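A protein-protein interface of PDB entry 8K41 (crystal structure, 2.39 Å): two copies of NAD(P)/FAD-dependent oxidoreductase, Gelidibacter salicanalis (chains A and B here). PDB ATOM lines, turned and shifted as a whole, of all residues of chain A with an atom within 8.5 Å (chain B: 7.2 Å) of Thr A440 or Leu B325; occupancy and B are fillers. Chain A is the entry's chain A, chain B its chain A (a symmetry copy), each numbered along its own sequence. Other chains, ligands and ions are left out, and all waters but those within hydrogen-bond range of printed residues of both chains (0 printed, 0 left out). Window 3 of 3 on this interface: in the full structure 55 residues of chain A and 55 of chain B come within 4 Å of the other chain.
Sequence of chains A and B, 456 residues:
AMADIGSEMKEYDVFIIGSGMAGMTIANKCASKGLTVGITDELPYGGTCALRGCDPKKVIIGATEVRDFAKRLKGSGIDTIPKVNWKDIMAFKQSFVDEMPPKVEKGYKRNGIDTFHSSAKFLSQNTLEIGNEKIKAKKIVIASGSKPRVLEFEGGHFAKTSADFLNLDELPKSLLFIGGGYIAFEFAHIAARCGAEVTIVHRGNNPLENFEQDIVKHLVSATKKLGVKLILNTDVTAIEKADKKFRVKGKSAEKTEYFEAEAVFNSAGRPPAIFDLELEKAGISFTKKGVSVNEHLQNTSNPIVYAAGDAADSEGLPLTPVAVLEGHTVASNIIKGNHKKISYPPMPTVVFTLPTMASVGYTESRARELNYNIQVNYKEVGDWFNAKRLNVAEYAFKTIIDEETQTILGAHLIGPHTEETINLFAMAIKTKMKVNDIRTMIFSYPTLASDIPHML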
ATOM      1  N   MET A 433      10.704 -17.229  -8.574  1.00  0.00           N
ATOM      2  CA  MET A 433      10.791 -16.066  -9.480  1.00  0.00           C
ATOM      3  C   MET A 433      12.126 -16.148 -10.221  1.00  0.00           C
ATOM      4  O   MET A 433      13.128 -16.473  -9.581  1.00  0.00           O
ATOM      5  CB  MET A 433      10.740 -14.785  -8.651  1.00  0.00           C
ATOM      6  CG  MET A 433      10.036 -13.633  -9.307  1.00  0.00           C
ATOM      7  SD  MET A 433       9.977 -12.272  -8.118  1.00  0.00           S
ATOM      8  CE  MET A 433       9.701 -10.893  -9.228  1.00  0.00           C
ATOM      9  N   LYS A 434      12.131 -15.878 -11.524  1.00  0.00           N
ATOM     10  CA  LYS A 434      13.362 -15.889 -12.347  1.00  0.00           C
ATOM     11  C   LYS A 434      14.144 -14.622 -12.036  1.00  0.00           C
ATOM     12  O   LYS A 434      13.525 -13.543 -11.863  1.00  0.00           O
ATOM     13  CB  LYS A 434      13.062 -15.933 -13.843  1.00  0.00           C
ATOM     14  CG  LYS A 434      12.166 -17.080 -14.262  1.00  0.00           C
ATOM     15  CD  LYS A 434      12.778 -18.408 -13.978  1.00  0.00           C
ATOM     16  CE  LYS A 434      12.175 -19.493 -14.838  1.00  0.00           C
ATOM     17  NZ  LYS A 434      12.896 -20.771 -14.657  1.00  0.00           N
ATOM     18  N   VAL A 435      15.462 -14.756 -12.033  1.00  0.00           N
ATOM     19  CA  VAL A 435      16.393 -13.657 -11.684  1.00  0.00           C
ATOM     20  C   VAL A 435      16.065 -12.432 -12.565  1.00  0.00           C
ATOM     21  O   VAL A 435      16.093 -11.306 -12.031  1.00  0.00           O
ATOM     22  CB  VAL A 435      17.838 -14.185 -11.786  1.00  0.00           C
ATOM     23  CG1 VAL A 435      18.872 -13.077 -11.775  1.00  0.00           C
ATOM     24  CG2 VAL A 435      18.125 -15.185 -10.671  1.00  0.00           C
ATOM     25  N   ASN A 436      15.680 -12.627 -13.831  1.00  0.00           N
ATOM     26  CA  ASN A 436      15.421 -11.506 -14.778  1.00  0.00           C
ATOM     27  C   ASN A 436      14.100 -10.809 -14.431  1.00  0.00           C
ATOM     28  O   ASN A 436      14.035  -9.565 -14.510  1.00  0.00           O
ATOM     29  CB  ASN A 436      15.405 -11.935 -16.244  1.00  0.00           C
ATOM     30  CG  ASN A 436      15.658 -10.740 -17.144  1.00  0.00           C
ATOM     31  OD1 ASN A 436      16.693 -10.081 -17.014  1.00  0.00           O
ATOM     32  ND2 ASN A 436      14.708 -10.411 -18.008  1.00  0.00           N
ATOM     33  N   ASP A 437      13.071 -11.580 -14.089  1.00  0.00           N
ATOM     34  CA  ASP A 437      11.767 -11.022 -13.655  1.00  0.00           C
ATOM     35  C   ASP A 437      12.076 -10.126 -12.448  1.00  0.00           C
ATOM     36  O   ASP A 437      11.502  -9.046 -12.372  1.00  0.00           O
ATOM     37  CB  ASP A 437      10.708 -12.110 -13.380  1.00  0.00           C
ATOM     38  CG  ASP A 437      10.363 -13.052 -14.541  1.00  0.00           C
ATOM     39  OD1 ASP A 437      10.959 -12.929 -15.636  1.00  0.00           O
ATOM     40  OD2 ASP A 437       9.513 -13.936 -14.336  1.00  0.00           O
ATOM     41  N   ILE A 438      12.991 -10.523 -11.554  1.00  0.00           N
ATOM     42  CA  ILE A 438      13.365  -9.675 -10.377  1.00  0.00           C
ATOM     43  C   ILE A 438      14.108  -8.432 -10.871  1.00  0.00           C
ATOM     44  O   ILE A 438      13.824  -7.343 -10.355  1.00  0.00           O
ATOM     45  CB  ILE A 438      14.206 -10.422  -9.323  1.00  0.00           C
ATOM     46  CG1 ILE A 438      13.514 -11.690  -8.826  1.00  0.00           C
ATOM     47  CG2 ILE A 438      14.558  -9.480  -8.177  1.00  0.00           C
ATOM     48  CD1 ILE A 438      14.403 -12.630  -8.044  1.00  0.00           C
ATOM     49  N   ARG A 439      15.057  -8.594 -11.792  1.00  0.00           N
ATOM     50  CA  ARG A 439      15.873  -7.465 -12.310  1.00  0.00           C
ATOM     51  C   ARG A 439      14.965  -6.415 -12.972  1.00  0.00           C
ATOM     52  O   ARG A 439      15.203  -5.237 -12.709  1.00  0.00           O
ATOM     53  CB  ARG A 439      16.981  -7.944 -13.256  1.00  0.00           C
ATOM     54  CG  ARG A 439      18.320  -8.183 -12.563  1.00  0.00           C
ATOM     55  CD  ARG A 439      19.482  -8.380 -13.524  1.00  0.00           C
ATOM     56  NE  ARG A 439      19.192  -9.442 -14.481  1.00  0.00           N
ATOM     57  CZ  ARG A 439      19.707 -10.673 -14.471  1.00  0.00           C
ATOM     58  NH1 ARG A 439      20.595 -11.041 -13.558  1.00  0.00           N
ATOM     59  NH2 ARG A 439      19.331 -11.536 -15.402  1.00  0.00           N
ATOM     60  N   THR A 440      13.945  -6.811 -13.741  1.00  0.00           N
ATOM     61  CA  THR A 440      13.080  -5.899 -14.553  1.00  0.00           C
ATOM     62  C   THR A 440      11.824  -5.428 -13.794  1.00  0.00           C
ATOM     63  O   THR A 440      11.034  -4.671 -14.381  1.00  0.00           O
ATOM     64  CB  THR A 440      12.624  -6.608 -15.827  1.00  0.00           C
ATOM     65  OG1 THR A 440      11.833  -7.715 -15.386  1.00  0.00           O
ATOM     66  CG2 THR A 440      13.794  -7.018 -16.695  1.00  0.00           C
ATOM     67  N   MET A 441      11.649  -5.878 -12.555  1.00  0.00           N
ATOM     68  CA  MET A 441      10.558  -5.525 -11.609  1.00  0.00           C
ATOM     69  C   MET A 441      10.818  -4.119 -11.062  1.00  0.00           C
ATOM     70  O   MET A 441      11.991  -3.679 -11.127  1.00  0.00           O
ATOM     71  CB  MET A 441      10.586  -6.504 -10.437  1.00  0.00           C
ATOM     72  CG  MET A 441       9.354  -6.537  -9.623  1.00  0.00           C
ATOM     73  SD  MET A 441       9.684  -7.459  -8.107  1.00  0.00           S
ATOM     74  CE  MET A 441       9.225  -6.163  -6.954  1.00  0.00           C
ATOM     75  N   ILE A 442       9.778  -3.437 -10.577  1.00  0.00           N
ATOM     76  CA  ILE A 442       9.907  -2.024 -10.124  1.00  0.00           C
ATOM     77  C   ILE A 442       9.693  -1.941  -8.617  1.00  0.00           C
ATOM     78  O   ILE A 442       8.656  -2.380  -8.116  1.00  0.00           O
ATOM     79  CB  ILE A 442       8.958  -1.059 -10.854  1.00  0.00           C
ATOM     80  CG1 ILE A 442       9.322  -0.927 -12.330  1.00  0.00           C
ATOM     81  CG2 ILE A 442       8.950   0.283 -10.112  1.00  0.00           C
ATOM     82  CD1 ILE A 442       8.588   0.180 -13.053  1.00  0.00           C
ATOM     83  N   PHE A 443      10.633  -1.289  -7.972  1.00  0.00           N
ATOM     84  CA  PHE A 443      10.631  -0.978  -6.535  1.00  0.00           C
ATOM     85  C   PHE A 443      10.335   0.507  -6.402  1.00  0.00           C
ATOM     86  O   PHE A 443      10.659   1.283  -7.308  1.00  0.00           O
ATOM     87  CB  PHE A 443      11.965  -1.423  -5.937  1.00  0.00           C
ATOM     88  CG  PHE A 443      12.199  -2.906  -6.089  1.00  0.00           C
ATOM     89  CD1 PHE A 443      12.524  -3.457  -7.315  1.00  0.00           C
ATOM     90  CD2 PHE A 443      12.023  -3.757  -5.015  1.00  0.00           C
ATOM     91  CE1 PHE A 443      12.692  -4.827  -7.453  1.00  0.00           C
ATOM     92  CE2 PHE A 443      12.218  -5.121  -5.147  1.00  0.00           C
ATOM     93  CZ  PHE A 443      12.539  -5.653  -6.366  1.00  0.00           C
ATOM     94  N   PRO A 453      17.815  -5.659  -7.227  1.00  0.00           N
ATOM     95  CA  PRO A 453      18.077  -6.013  -8.623  1.00  0.00           C
ATOM     96  C   PRO A 453      19.594  -6.056  -8.880  1.00  0.00           C
ATOM     97  O   PRO A 453      20.072  -6.841  -9.692  1.00  0.00           O
ATOM     98  CB  PRO A 453      17.387  -4.873  -9.413  1.00  0.00           C
ATOM     99  CG  PRO A 453      16.312  -4.346  -8.470  1.00  0.00           C
ATOM    100  CD  PRO A 453      16.931  -4.486  -7.095  1.00  0.00           C
ATOM    101  N   MET B  21      17.559   9.961 -15.654  1.00  0.00           N
ATOM    102  CA  MET B  21      17.532   8.479 -15.565  1.00  0.00           C
ATOM    103  C   MET B  21      17.298   7.846 -16.947  1.00  0.00           C
ATOM    104  O   MET B  21      17.978   6.864 -17.249  1.00  0.00           O
ATOM    105  CB  MET B  21      16.422   8.042 -14.610  1.00  0.00           C
ATOM    106  CG  MET B  21      16.623   8.531 -13.201  1.00  0.00           C
ATOM    107  SD  MET B  21      18.189   8.001 -12.450  1.00  0.00           S
ATOM    108  CE  MET B  21      18.422   6.373 -13.168  1.00  0.00           C
ATOM    109  N   ALA B  22      16.348   8.380 -17.730  1.00  0.00           N
ATOM    110  CA  ALA B  22      15.904   7.867 -19.049  1.00  0.00           C
ATOM    111  C   ALA B  22      17.026   8.004 -20.087  1.00  0.00           C
ATOM    112  O   ALA B  22      17.410   6.971 -20.732  1.00  0.00           O
ATOM    113  CB  ALA B  22      14.670   8.623 -19.487  1.00  0.00           C
ATOM    114  N   THR B  25      20.290   5.986 -19.187  1.00  0.00           N
ATOM    115  CA  THR B  25      20.009   4.547 -19.404  1.00  0.00           C
ATOM    116  C   THR B  25      20.204   4.207 -20.884  1.00  0.00           C
ATOM    117  O   THR B  25      20.774   3.131 -21.177  1.00  0.00           O
ATOM    118  CB  THR B  25      18.579   4.219 -18.974  1.00  0.00           C
ATOM    119  OG1 THR B  25      18.507   4.508 -17.584  1.00  0.00           O
ATOM    120  CG2 THR B  25      18.173   2.792 -19.250  1.00  0.00           C
ATOM    121  N   LEU B 297       7.230   2.766 -27.623  1.00  0.00           N
ATOM    122  CA  LEU B 297       7.632   4.111 -27.118  1.00  0.00           C
ATOM    123  C   LEU B 297       8.172   4.979 -28.266  1.00  0.00           C
ATOM    124  O   LEU B 297       9.005   5.840 -28.012  1.00  0.00           O
ATOM    125  CB  LEU B 297       8.640   3.939 -25.973  1.00  0.00           C
ATOM    126  CG  LEU B 297       8.061   3.290 -24.711  1.00  0.00           C
ATOM    127  CD1 LEU B 297       9.070   3.307 -23.573  1.00  0.00           C
ATOM    128  CD2 LEU B 297       6.792   3.998 -24.259  1.00  0.00           C
ATOM    129  N   ALA B 308      10.802   8.658 -23.315  1.00  0.00           N
ATOM    130  CA  ALA B 308      10.955   7.841 -22.091  1.00  0.00           C
ATOM    131  C   ALA B 308      11.052   8.759 -20.869  1.00  0.00           C
ATOM    132  O   ALA B 308      11.738   9.798 -20.955  1.00  0.00           O
ATOM    133  CB  ALA B 308      12.166   6.946 -22.215  1.00  0.00           C
ATOM    134  N   LEU B 319       8.156   8.482 -12.259  1.00  0.00           N
ATOM    135  CA  LEU B 319       9.022   7.981 -11.144  1.00  0.00           C
ATOM    136  C   LEU B 319      10.382   7.527 -11.689  1.00  0.00           C
ATOM    137  O   LEU B 319      10.486   7.112 -12.871  1.00  0.00           O
ATOM    138  CB  LEU B 319       8.360   6.784 -10.443  1.00  0.00           C
ATOM    139  CG  LEU B 319       6.971   6.991  -9.823  1.00  0.00           C
ATOM    140  CD1 LEU B 319       6.306   5.647  -9.601  1.00  0.00           C
ATOM    141  CD2 LEU B 319       7.046   7.749  -8.500  1.00  0.00           C
ATOM    142  N   THR B 320      11.393   7.527 -10.830  1.00  0.00           N
ATOM    143  CA  THR B 320      12.785   7.210 -11.213  1.00  0.00           C
ATOM    144  C   THR B 320      12.816   5.802 -11.817  1.00  0.00           C
ATOM    145  O   THR B 320      13.224   5.619 -12.958  1.00  0.00           O
ATOM    146  CB  THR B 320      13.682   7.490 -10.005  1.00  0.00           C
ATOM    147  OG1 THR B 320      13.696   8.913  -9.885  1.00  0.00           O
ATOM    148  CG2 THR B 320      15.075   6.927 -10.153  1.00  0.00           C
ATOM    149  N   PRO B 321      12.337   4.749 -11.129  1.00  0.00           N
ATOM    150  CA  PRO B 321      12.423   3.400 -11.683  1.00  0.00           C
ATOM    151  C   PRO B 321      11.676   3.238 -13.012  1.00  0.00           C
ATOM    152  O   PRO B 321      12.068   2.367 -13.751  1.00  0.00           O
ATOM    153  CB  PRO B 321      11.776   2.498 -10.627  1.00  0.00           C
ATOM    154  CG  PRO B 321      11.829   3.327  -9.356  1.00  0.00           C
ATOM    155  CD  PRO B 321      11.716   4.771  -9.798  1.00  0.00           C
ATOM    156  N   VAL B 322      10.640   4.053 -13.268  1.00  0.00           N
ATOM    157  CA  VAL B 322       9.808   3.977 -14.513  1.00  0.00           C
ATOM    158  C   VAL B 322      10.588   4.535 -15.703  1.00  0.00           C
ATOM    159  O   VAL B 322      10.490   3.937 -16.801  1.00  0.00           O
ATOM    160  CB  VAL B 322       8.466   4.713 -14.369  1.00  0.00           C
ATOM    161  CG1 VAL B 322       7.670   4.711 -15.684  1.00  0.00           C
ATOM    162  CG2 VAL B 322       7.641   4.114 -13.238  1.00  0.00           C
ATOM    163  N   ALA B 323      11.335   5.629 -15.497  1.00  0.00           N
ATOM    164  CA  ALA B 323      12.179   6.291 -16.523  1.00  0.00           C
ATOM    165  C   ALA B 323      13.215   5.284 -17.017  1.00  0.00           C
ATOM    166  O   ALA B 323      13.514   5.265 -18.243  1.00  0.00           O
ATOM    167  CB  ALA B 323      12.819   7.539 -15.954  1.00  0.00           C
ATOM    168  N   VAL B 324      13.725   4.457 -16.100  1.00  0.00           N
ATOM    169  CA  VAL B 324      14.736   3.415 -16.430  1.00  0.00           C
ATOM    170  C   VAL B 324      14.068   2.348 -17.307  1.00  0.00           C
ATOM    171  O   VAL B 324      14.681   1.990 -18.305  1.00  0.00           O
ATOM    172  CB  VAL B 324      15.409   2.771 -15.196  1.00  0.00           C
ATOM    173  CG1 VAL B 324      16.234   1.556 -15.604  1.00  0.00           C
ATOM    174  CG2 VAL B 324      16.282   3.748 -14.423  1.00  0.00           C
ATOM    175  N   LEU B 325      12.912   1.805 -16.916  1.00  0.00           N
ATOM    176  CA  LEU B 325      12.309   0.635 -17.614  1.00  0.00           C
ATOM    177  C   LEU B 325      11.902   1.073 -19.024  1.00  0.00           C
ATOM    178  O   LEU B 325      12.100   0.274 -19.966  1.00  0.00           O
ATOM    179  CB  LEU B 325      11.113   0.120 -16.810  1.00  0.00           C
ATOM    180  CG  LEU B 325      10.277  -0.970 -17.496  1.00  0.00           C
ATOM    181  CD1 LEU B 325      10.735  -2.375 -17.107  1.00  0.00           C
ATOM    182  CD2 LEU B 325       8.798  -0.796 -17.179  1.00  0.00           C
ATOM    183  N   GLU B 326      11.398   2.314 -19.149  1.00  0.00           N
ATOM    184  CA  GLU B 326      11.033   2.968 -20.437  1.00  0.00           C
ATOM    185  C   GLU B 326      12.311   3.191 -21.259  1.00  0.00           C
ATOM    186  O   GLU B 326      12.279   2.970 -22.488  1.00  0.00           O
ATOM    187  CB  GLU B 326      10.230   4.251 -20.170  1.00  0.00           C
ATOM    188  CG  GLU B 326       8.794   3.982 -19.729  1.00  0.00           C
ATOM    189  CD  GLU B 326       7.869   5.184 -19.586  1.00  0.00           C
ATOM    190  OE1 GLU B 326       6.634   4.967 -19.354  1.00  0.00           O
ATOM    191  OE2 GLU B 326       8.362   6.334 -19.708  1.00  0.00           O
ATOM    192  N   GLY B 327      13.412   3.578 -20.606  1.00  0.00           N
ATOM    193  CA  GLY B 327      14.740   3.661 -21.248  1.00  0.00           C
ATOM    194  C   GLY B 327      15.082   2.402 -22.036  1.00  0.00           C
ATOM    195  O   GLY B 327      15.389   2.537 -23.218  1.00  0.00           O
ATOM    196  N   HIS B 328      15.004   1.226 -21.400  1.00  0.00           N
ATOM    197  CA  HIS B 328      15.475  -0.090 -21.912  1.00  0.00           C
ATOM    198  C   HIS B 328      14.695  -0.534 -23.164  1.00  0.00           C
ATOM    199  O   HIS B 328      15.318  -1.119 -24.050  1.00  0.00           O
ATOM    200  CB  HIS B 328      15.423  -1.149 -20.798  1.00  0.00           C
ATOM    201  CG  HIS B 328      16.589  -1.063 -19.872  1.00  0.00           C
ATOM    202  ND1 HIS B 328      17.894  -1.010 -20.334  1.00  0.00           N
ATOM    203  CD2 HIS B 328      16.666  -1.005 -18.526  1.00  0.00           C
ATOM    204  CE1 HIS B 328      18.718  -0.914 -19.314  1.00  0.00           C
ATOM    205  NE2 HIS B 328      17.991  -0.910 -18.197  1.00  0.00           N
ATOM    206  N   THR B 329      13.397  -0.270 -23.229  1.00  0.00           N
ATOM    207  CA  THR B 329      12.550  -0.562 -24.406  1.00  0.00           C
ATOM    208  C   THR B 329      12.980   0.343 -25.572  1.00  0.00           C
ATOM    209  O   THR B 329      13.167  -0.188 -26.677  1.00  0.00           O
ATOM    210  CB  THR B 329      11.071  -0.446 -24.027  1.00  0.00           C
ATOM    211  OG1 THR B 329      10.843  -1.468 -23.057  1.00  0.00           O
ATOM    212  CG2 THR B 329      10.133  -0.610 -25.205  1.00  0.00           C
ATOM    213  N   VAL B 330      13.142   1.647 -25.330  1.00  0.00           N
ATOM    214  CA  VAL B 330      13.575   2.634 -26.360  1.00  0.00           C
ATOM    215  C   VAL B 330      14.960   2.217 -26.862  1.00  0.00           C
ATOM    216  O   VAL B 330      15.085   1.905 -28.061  1.00  0.00           O
ATOM    217  CB  VAL B 330      13.582   4.069 -25.799  1.00  0.00           C
ATOM    218  CG1 VAL B 330      14.391   5.027 -26.668  1.00  0.00           C
ATOM    219  CG2 VAL B 330      12.173   4.592 -25.584  1.00  0.00           C
ATOM    220  N   LYS B 340      10.325  -4.885 -29.496  1.00  0.00           N
ATOM    221  CA  LYS B 340       9.988  -4.973 -28.055  1.00  0.00           C
ATOM    222  C   LYS B 340       8.882  -3.948 -27.737  1.00  0.00           C
ATOM    223  O   LYS B 340       9.074  -2.754 -28.047  1.00  0.00           O
ATOM    224  CB  LYS B 340      11.294  -4.731 -27.290  1.00  0.00           C
ATOM    225  CG  LYS B 340      11.187  -4.467 -25.798  1.00  0.00           C
ATOM    226  CD  LYS B 340      11.460  -5.690 -24.962  1.00  0.00           C
ATOM    227  CE  LYS B 340      11.720  -5.346 -23.510  1.00  0.00           C
ATOM    228  NZ  LYS B 340      13.020  -4.650 -23.350  1.00  0.00           N
ATOM    229  N   ILE B 342       6.662  -2.055 -24.661  1.00  0.00           N
ATOM    230  CA  ILE B 342       6.829  -1.693 -23.225  1.00  0.00           C
ATOM    231  C   ILE B 342       5.775  -2.466 -22.430  1.00  0.00           C
ATOM    232  O   ILE B 342       4.605  -2.479 -22.853  1.00  0.00           O
ATOM    233  CB  ILE B 342       6.747  -0.177 -22.967  1.00  0.00           C
ATOM    234  CG1 ILE B 342       6.991   0.153 -21.492  1.00  0.00           C
ATOM    235  CG2 ILE B 342       5.422   0.420 -23.437  1.00  0.00           C
ATOM    236  CD1 ILE B 342       8.352  -0.202 -20.992  1.00  0.00           C
ATOM    237  N   SER B 343       6.206  -3.100 -21.336  1.00  0.00           N
ATOM    238  CA  SER B 343       5.373  -3.876 -20.394  1.00  0.00           C
ATOM    239  C   SER B 343       5.653  -3.342 -18.988  1.00  0.00           C
ATOM    240  O   SER B 343       6.834  -3.344 -18.581  1.00  0.00           O
ATOM    241  CB  SER B 343       5.670  -5.350 -20.543  1.00  0.00           C
ATOM    242  OG  SER B 343       5.125  -6.105 -19.473  1.00  0.00           O
ATOM    243  N   TYR B 344       4.616  -2.870 -18.291  1.00  0.00           N
ATOM    244  CA  TYR B 344       4.707  -2.307 -16.921  1.00  0.00           C
ATOM    245  C   TYR B 344       4.370  -3.371 -15.879  1.00  0.00           C
ATOM    246  O   TYR B 344       3.269  -3.911 -15.875  1.00  0.00           O
ATOM    247  CB  TYR B 344       3.786  -1.094 -16.795  1.00  0.00           C
ATOM    248  CG  TYR B 344       4.145   0.022 -17.741  1.00  0.00           C
ATOM    249  CD1 TYR B 344       3.602   0.081 -19.013  1.00  0.00           C
ATOM    250  CD2 TYR B 344       5.073   0.988 -17.381  1.00  0.00           C
ATOM    251  CE1 TYR B 344       3.956   1.078 -19.902  1.00  0.00           C
ATOM    252  CE2 TYR B 344       5.424   2.007 -18.251  1.00  0.00           C
ATOM    253  CZ  TYR B 344       4.863   2.050 -19.516  1.00  0.00           C
ATOM    254  OH  TYR B 344       5.213   3.026 -20.396  1.00  0.00           O
ATOM    255  N   PRO B 345       5.278  -3.672 -14.923  1.00  0.00           N
ATOM    256  CA  PRO B 345       4.893  -4.398 -13.713  1.00  0.00           C
ATOM    257  C   PRO B 345       4.208  -3.481 -12.702  1.00  0.00           C
ATOM    258  O   PRO B 345       4.038  -2.282 -12.944  1.00  0.00           O
ATOM    259  CB  PRO B 345       6.246  -4.924 -13.212  1.00  0.00           C
ATOM    260  CG  PRO B 345       7.220  -3.848 -13.610  1.00  0.00           C
ATOM    261  CD  PRO B 345       6.710  -3.347 -14.945  1.00  0.00           C
ATOM    262  N   MET B 347       3.794  -0.811 -10.007  1.00  0.00           N
ATOM    263  CA  MET B 347       4.587   0.432  -9.900  1.00  0.00           C
ATOM    264  C   MET B 347       4.403   0.979  -8.493  1.00  0.00           C
ATOM    265  O   MET B 347       3.618   1.891  -8.278  1.00  0.00           O
ATOM    266  CB  MET B 347       4.134   1.452 -10.948  1.00  0.00           C
ATOM    267  CG  MET B 347       4.664   1.128 -12.329  1.00  0.00           C
ATOM    268  SD  MET B 347       4.212   2.317 -13.643  1.00  0.00           S
ATOM    269  CE  MET B 347       2.730   1.503 -14.243  1.00  0.00           C
ATOM    270  N   LYS B 430       2.902  -9.277  -8.947  1.00  0.00           N
ATOM    271  CA  LYS B 430       3.634  -9.678 -10.188  1.00  0.00           C
ATOM    272  C   LYS B 430       3.715 -11.202 -10.300  1.00  0.00           C
ATOM    273  O   LYS B 430       3.602 -11.715 -11.417  1.00  0.00           O
ATOM    274  CB  LYS B 430       5.066  -9.142 -10.246  1.00  0.00           C
ATOM    275  CG  LYS B 430       5.908  -9.728 -11.387  1.00  0.00           C
ATOM    276  CD  LYS B 430       7.002  -8.810 -11.931  1.00  0.00           C
ATOM    277  CE  LYS B 430       7.553  -9.223 -13.287  1.00  0.00           C
ATOM    278  NZ  LYS B 430       6.507  -9.739 -14.208  1.00  0.00           N
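O of Asn A436 is in hydrogen-bond range of OG1 of Thr A440 (3.0 Å).
The side-chain hydroxyl (OG1) of Thr A440 lies within hydrogen-bond range of the backbone carbonyl oxygen (O) of Asp A437 (3.3 Å).
CD1 of Leu B325 touches O of Thr A440, 3.6 Å away.
Thr A440 touches Pro B345.
CG2 of Ile A442 touches CB of Pro B321, 3.6 Å away.
CG1 of Ile A442 touches CG of Pro B345, at 3.8 Å.
Phe A443 touches Pro B321 (O to CG, 3.1 Å).
Lys A434 touches none of the printed residues of chain B.
Thr A440 touches just these residues of chain B: Leu B325 (3.6 Å) and Pro B345 (3.98 Å).
Of the printed residues of chain B, Ile A442 touches Pro B321 (3.6 Å) and Pro B345 (3.8 Å).
Of the printed residues of chain B, Phe A443 touches Pro B321 (3.1 Å).
Of the printed residues of chain A, Pro B321 touches Ile A442 and Phe A443.
Leu B325 touches just one residue of chain A: Thr A440 (3.6 Å).
Of the printed residues of chain A, Pro B345 touches Thr A440 and Ile A442.
Lys B430 touches none of the printed residues of chain A.
Of the 12 printed residues of chain A, 3 touch a printed residue of chain B.
Printed residues of chain A that touch a printed residue of chain B: Thr A440, Ile A442 and Phe A443.
Among the printed residues, 5 pairs touch across the chains.
Among the printed residues, no Asp or Glu carboxylate lies within 4 Å of a Lys or Arg side-chain nitrogen of the other chain.
No position is printed for both chains.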
